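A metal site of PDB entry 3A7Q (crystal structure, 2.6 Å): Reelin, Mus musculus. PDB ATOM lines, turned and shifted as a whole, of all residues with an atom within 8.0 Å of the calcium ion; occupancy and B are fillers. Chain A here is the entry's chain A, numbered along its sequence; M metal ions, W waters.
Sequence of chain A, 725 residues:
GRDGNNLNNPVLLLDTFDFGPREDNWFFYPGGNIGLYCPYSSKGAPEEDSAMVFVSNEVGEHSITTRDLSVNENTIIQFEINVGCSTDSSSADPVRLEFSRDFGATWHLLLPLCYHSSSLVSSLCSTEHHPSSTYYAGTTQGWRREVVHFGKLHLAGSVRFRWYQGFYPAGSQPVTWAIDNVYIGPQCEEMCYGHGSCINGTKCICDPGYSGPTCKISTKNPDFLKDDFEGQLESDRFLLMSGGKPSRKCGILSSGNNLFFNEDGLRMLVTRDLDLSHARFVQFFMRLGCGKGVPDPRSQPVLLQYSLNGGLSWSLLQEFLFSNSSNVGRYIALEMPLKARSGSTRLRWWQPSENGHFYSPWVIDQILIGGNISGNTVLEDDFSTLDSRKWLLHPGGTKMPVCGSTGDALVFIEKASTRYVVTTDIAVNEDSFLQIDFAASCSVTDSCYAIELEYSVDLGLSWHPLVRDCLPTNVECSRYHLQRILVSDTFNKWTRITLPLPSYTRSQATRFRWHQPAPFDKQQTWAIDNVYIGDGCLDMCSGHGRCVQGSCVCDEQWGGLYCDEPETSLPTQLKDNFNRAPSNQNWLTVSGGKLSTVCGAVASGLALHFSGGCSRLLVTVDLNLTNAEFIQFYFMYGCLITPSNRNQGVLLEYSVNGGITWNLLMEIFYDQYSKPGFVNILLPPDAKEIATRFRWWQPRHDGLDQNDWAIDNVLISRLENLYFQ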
ATOM      1  N   ASP A 381      -0.527 -20.459   7.960  1.00  0.00           N
ATOM      2  CA  ASP A 381      -0.370 -19.579   6.797  1.00  0.00           C
ATOM      3  C   ASP A 381       1.085 -19.246   6.405  1.00  0.00           C
ATOM      4  O   ASP A 381       1.923 -18.989   7.268  1.00  0.00           O
ATOM      5  CB  ASP A 381      -1.193 -18.291   7.008  1.00  0.00           C
ATOM      6  CG  ASP A 381      -1.876 -17.813   5.727  1.00  0.00           C
ATOM      7  OD1 ASP A 381      -1.326 -18.004   4.620  1.00  0.00           O
ATOM      8  OD2 ASP A 381      -2.966 -17.225   5.832  1.00  0.00           O
ATOM      9  N   ASP A 382       1.370 -19.280   5.103  1.00  0.00           N
ATOM     10  CA  ASP A 382       2.623 -18.736   4.564  1.00  0.00           C
ATOM     11  C   ASP A 382       2.386 -17.453   3.735  1.00  0.00           C
ATOM     12  O   ASP A 382       3.336 -16.850   3.189  1.00  0.00           O
ATOM     13  CB  ASP A 382       3.416 -19.803   3.791  1.00  0.00           C
ATOM     14  CG  ASP A 382       2.811 -20.148   2.433  1.00  0.00           C
ATOM     15  OD1 ASP A 382       1.647 -19.801   2.149  1.00  0.00           O
ATOM     16  OD2 ASP A 382       3.508 -20.781   1.606  1.00  0.00           O
ATOM     17  N   PHE A 383       1.117 -17.042   3.678  1.00  0.00           N
ATOM     18  CA  PHE A 383       0.641 -15.879   2.913  1.00  0.00           C
ATOM     19  C   PHE A 383       1.049 -15.862   1.450  1.00  0.00           C
ATOM     20  O   PHE A 383       1.481 -14.830   0.956  1.00  0.00           O
ATOM     21  CB  PHE A 383       1.056 -14.534   3.550  1.00  0.00           C
ATOM     22  CG  PHE A 383       0.634 -14.383   4.974  1.00  0.00           C
ATOM     23  CD1 PHE A 383      -0.671 -14.031   5.285  1.00  0.00           C
ATOM     24  CD2 PHE A 383       1.550 -14.576   5.996  1.00  0.00           C
ATOM     25  CE1 PHE A 383      -1.071 -13.890   6.627  1.00  0.00           C
ATOM     26  CE2 PHE A 383       1.162 -14.418   7.329  1.00  0.00           C
ATOM     27  CZ  PHE A 383      -0.146 -14.086   7.644  1.00  0.00           C
ATOM     28  N   SER A 384       0.907 -16.986   0.762  1.00  0.00           N
ATOM     29  CA  SER A 384       0.969 -16.992  -0.683  1.00  0.00           C
ATOM     30  C   SER A 384      -0.354 -16.402  -1.177  1.00  0.00           C
ATOM     31  O   SER A 384      -0.419 -15.782  -2.243  1.00  0.00           O
ATOM     32  CB  SER A 384       1.207 -18.411  -1.222  1.00  0.00           C
ATOM     33  OG  SER A 384       0.043 -19.247  -1.113  1.00  0.00           O
ATOM     34  N   THR A 385      -1.400 -16.619  -0.387  1.00  0.00           N
ATOM     35  CA  THR A 385      -2.715 -16.042  -0.604  1.00  0.00           C
ATOM     36  C   THR A 385      -3.133 -15.376   0.720  1.00  0.00           C
ATOM     37  O   THR A 385      -2.527 -15.630   1.757  1.00  0.00           O
ATOM     38  CB  THR A 385      -3.758 -17.128  -0.994  1.00  0.00           C
ATOM     39  OG1 THR A 385      -3.919 -18.044   0.094  1.00  0.00           O
ATOM     40  CG2 THR A 385      -3.318 -17.919  -2.220  1.00  0.00           C
ATOM     41  N   MET A 400       2.436  -8.855   0.528  1.00  0.00           N
ATOM     42  CA  MET A 400       3.637  -8.480  -0.201  1.00  0.00           C
ATOM     43  C   MET A 400       4.834  -9.118   0.513  1.00  0.00           C
ATOM     44  O   MET A 400       4.725  -9.487   1.679  1.00  0.00           O
ATOM     45  CB  MET A 400       3.782  -6.951  -0.250  1.00  0.00           C
ATOM     46  CG  MET A 400       3.746  -6.276   1.107  1.00  0.00           C
ATOM     47  SD  MET A 400       3.966  -4.493   1.037  1.00  0.00           S
ATOM     48  CE  MET A 400       5.663  -4.357   0.451  1.00  0.00           C
ATOM     49  N   PRO A 401       5.960  -9.257  -0.203  1.00  0.00           N
ATOM     50  CA  PRO A 401       7.196  -9.582   0.502  1.00  0.00           C
ATOM     51  C   PRO A 401       7.752  -8.337   1.188  1.00  0.00           C
ATOM     52  O   PRO A 401       7.454  -7.214   0.767  1.00  0.00           O
ATOM     53  CB  PRO A 401       8.141 -10.015  -0.625  1.00  0.00           C
ATOM     54  CG  PRO A 401       7.638  -9.325  -1.820  1.00  0.00           C
ATOM     55  CD  PRO A 401       6.157  -9.169  -1.658  1.00  0.00           C
ATOM     56  N   SER A 405      11.832 -11.847   3.031  1.00  0.00           N
ATOM     57  CA  SER A 405      10.919 -12.928   3.392  1.00  0.00           C
ATOM     58  C   SER A 405      10.826 -14.021   2.310  1.00  0.00           C
ATOM     59  O   SER A 405      11.307 -13.850   1.167  1.00  0.00           O
ATOM     60  CB  SER A 405       9.536 -12.347   3.668  1.00  0.00           C
ATOM     61  OG  SER A 405       9.042 -11.702   2.510  1.00  0.00           O
ATOM     62  N   THR A 406      10.203 -15.129   2.680  1.00  0.00           N
ATOM     63  CA  THR A 406       9.906 -16.203   1.750  1.00  0.00           C
ATOM     64  C   THR A 406       8.505 -15.969   1.189  1.00  0.00           C
ATOM     65  O   THR A 406       7.495 -16.039   1.914  1.00  0.00           O
ATOM     66  CB  THR A 406      10.046 -17.584   2.404  1.00  0.00           C
ATOM     67  OG1 THR A 406      11.144 -17.553   3.335  1.00  0.00           O
ATOM     68  CG2 THR A 406      10.293 -18.675   1.346  1.00  0.00           C
ATOM     69  N   GLY A 407       8.477 -15.683  -0.106  1.00  0.00           N
ATOM     70  CA  GLY A 407       7.262 -15.217  -0.773  1.00  0.00           C
ATOM     71  C   GLY A 407       6.712 -13.968  -0.109  1.00  0.00           C
ATOM     72  O   GLY A 407       7.457 -13.097   0.346  1.00  0.00           O
ATOM     73  N   ASP A 408       5.400 -13.892  -0.069  1.00  0.00           N
ATOM     74  CA  ASP A 408       4.700 -12.805   0.565  1.00  0.00           C
ATOM     75  C   ASP A 408       4.568 -13.024   2.072  1.00  0.00           C
ATOM     76  O   ASP A 408       4.506 -14.157   2.563  1.00  0.00           O
ATOM     77  CB  ASP A 408       3.310 -12.636  -0.051  1.00  0.00           C
ATOM     78  CG  ASP A 408       3.341 -12.029  -1.450  1.00  0.00           C
ATOM     79  OD1 ASP A 408       4.435 -11.900  -2.046  1.00  0.00           O
ATOM     80  OD2 ASP A 408       2.246 -11.687  -1.947  1.00  0.00           O
ATOM     81  N   ALA A 409       4.522 -11.893   2.774  1.00  0.00           N
ATOM     82  CA  ALA A 409       4.097 -11.821   4.165  1.00  0.00           C
ATOM     83  C   ALA A 409       2.870 -10.904   4.232  1.00  0.00           C
ATOM     84  O   ALA A 409       2.510 -10.257   3.252  1.00  0.00           O
ATOM     85  CB  ALA A 409       5.214 -11.272   5.021  1.00  0.00           C
ATOM     86  N   LEU A 410       2.207 -10.894   5.385  1.00  0.00           N
ATOM     87  CA  LEU A 410       1.209  -9.885   5.679  1.00  0.00           C
ATOM     88  C   LEU A 410       1.985  -8.710   6.224  1.00  0.00           C
ATOM     89  O   LEU A 410       2.666  -8.844   7.235  1.00  0.00           O
ATOM     90  CB  LEU A 410       0.223 -10.414   6.724  1.00  0.00           C
ATOM     91  CG  LEU A 410      -0.891  -9.473   7.201  1.00  0.00           C
ATOM     92  CD1 LEU A 410      -1.694  -8.938   6.016  1.00  0.00           C
ATOM     93  CD2 LEU A 410      -1.785 -10.186   8.219  1.00  0.00           C
ATOM     94  N   ASP A 437       6.697 -15.778  12.248  1.00  0.00           N
ATOM     95  CA  ASP A 437       7.871 -14.977  11.939  1.00  0.00           C
ATOM     96  C   ASP A 437       7.415 -13.528  12.064  1.00  0.00           C
ATOM     97  O   ASP A 437       6.325 -13.189  11.599  1.00  0.00           O
ATOM     98  CB  ASP A 437       8.379 -15.230  10.526  1.00  0.00           C
ATOM     99  CG  ASP A 437       9.199 -16.497  10.408  1.00  0.00           C
ATOM    100  OD1 ASP A 437       9.390 -17.207  11.426  1.00  0.00           O
ATOM    101  OD2 ASP A 437       9.659 -16.774   9.283  1.00  0.00           O
ATOM    102  N   TRP A 494      13.581 -10.484  10.303  1.00  0.00           N
ATOM    103  CA  TRP A 494      12.845 -11.728  10.549  1.00  0.00           C
ATOM    104  C   TRP A 494      13.407 -12.562  11.684  1.00  0.00           C
ATOM    105  O   TRP A 494      14.583 -12.914  11.716  1.00  0.00           O
ATOM    106  CB  TRP A 494      12.708 -12.569   9.270  1.00  0.00           C
ATOM    107  CG  TRP A 494      11.782 -11.956   8.274  1.00  0.00           C
ATOM    108  CD1 TRP A 494      12.111 -11.487   7.036  1.00  0.00           C
ATOM    109  CD2 TRP A 494      10.384 -11.716   8.445  1.00  0.00           C
ATOM    110  NE1 TRP A 494      11.003 -10.973   6.417  1.00  0.00           N
ATOM    111  CE2 TRP A 494       9.926 -11.102   7.259  1.00  0.00           C
ATOM    112  CE3 TRP A 494       9.468 -11.971   9.469  1.00  0.00           C
ATOM    113  CZ2 TRP A 494       8.589 -10.732   7.074  1.00  0.00           C
ATOM    114  CZ3 TRP A 494       8.149 -11.600   9.296  1.00  0.00           C
ATOM    115  CH2 TRP A 494       7.726 -10.990   8.113  1.00  0.00           C
ATOM    116  N   ILE A 528       4.200 -10.031   9.545  1.00  0.00           N
ATOM    117  CA  ILE A 528       4.168 -11.424   9.998  1.00  0.00           C
ATOM    118  C   ILE A 528       4.171 -12.381   8.794  1.00  0.00           C
ATOM    119  O   ILE A 528       3.709 -12.021   7.717  1.00  0.00           O
ATOM    120  CB  ILE A 528       2.946 -11.707  10.901  1.00  0.00           C
ATOM    121  CG1 ILE A 528       1.653 -11.419  10.130  1.00  0.00           C
ATOM    122  CG2 ILE A 528       3.000 -10.832  12.141  1.00  0.00           C
ATOM    123  CD1 ILE A 528       0.420 -12.144  10.660  1.00  0.00           C
ATOM    124  N   ASP A 529       4.701 -13.579   9.010  1.00  0.00           N
ATOM    125  CA  ASP A 529       4.765 -14.629   7.982  1.00  0.00           C
ATOM    126  C   ASP A 529       4.834 -15.957   8.740  1.00  0.00           C
ATOM    127  O   ASP A 529       5.023 -15.941   9.957  1.00  0.00           O
ATOM    128  CB  ASP A 529       6.014 -14.450   7.091  1.00  0.00           C
ATOM    129  CG  ASP A 529       5.915 -15.196   5.753  1.00  0.00           C
ATOM    130  OD1 ASP A 529       5.004 -16.020   5.550  1.00  0.00           O
ATOM    131  OD2 ASP A 529       6.788 -14.934   4.881  1.00  0.00           O
ATOM    132  N   ASN A 530       4.655 -17.081   8.028  1.00  0.00           N
ATOM    133  CA  ASN A 530       4.852 -18.444   8.565  1.00  0.00           C
ATOM    134  C   ASN A 530       4.140 -18.643   9.916  1.00  0.00           C
ATOM    135  O   ASN A 530       4.733 -19.053  10.936  1.00  0.00           O
ATOM    136  CB  ASN A 530       6.355 -18.793   8.616  1.00  0.00           C
ATOM    137  CG  ASN A 530       7.050 -18.650   7.236  1.00  0.00           C
ATOM    138  OD1 ASN A 530       6.529 -19.089   6.203  1.00  0.00           O
ATOM    139  ND2 ASN A 530       8.219 -18.060   7.229  1.00  0.00           N
ATOM    140  N   VAL A 531       2.850 -18.332   9.910  1.00  0.00           N
ATOM    141  CA  VAL A 531       2.011 -18.419  11.085  1.00  0.00           C
ATOM    142  C   VAL A 531       1.510 -19.836  11.243  1.00  0.00           C
ATOM    143  O   VAL A 531       0.857 -20.351  10.345  1.00  0.00           O
ATOM    144  CB  VAL A 531       0.789 -17.497  10.987  1.00  0.00           C
ATOM    145  CG1 VAL A 531      -0.171 -17.743  12.163  1.00  0.00           C
ATOM    146  CG2 VAL A 531       1.225 -16.044  10.907  1.00  0.00           C
HETATM  147 CA    CA M   1       5.576 -16.113   3.262  1.00  0.00          CA
HETATM  148  O   HOH W   1       6.693 -18.084   3.690  1.00  0.00           O
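Within 4 Å of the calcium ion: Asp 382, Thr 406, Asp 408 and Asp 529.
The nearest printed residue that does not touch the calcium ion is Gly 407 (4.2 Å).
The backbone NH (N) of Asp 437 sits at hydrogen-bond distance from the backbone carbonyl oxygen (O) of Asp 529, at 2.8 Å.
The side-chain carboxylate (OD1) of Asp 382 lies within hydrogen-bond range of the backbone NH (N) of Ser 384, 3.2 Å away.
The side-chain amide oxygen (OD1) of Asn 530 sits close to the side-chain carboxylate (OD1) of Asp 529, at 3.5 Å.
The calcium ion is bound by water W1 (2.3 Å), the backbone carbonyl oxygen (O) of Asp 408 (2.3 Å), the side-chain carboxylate (OD2) of Asp 529 (2.3 Å), the backbone carbonyl oxygen (O) of Thr 406 (2.3 Å), the backbone carbonyl oxygen (O) of Asp 382 (2.4 Å) and the side-chain carboxylate (OD1) of Asp 529 (2.4 Å).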
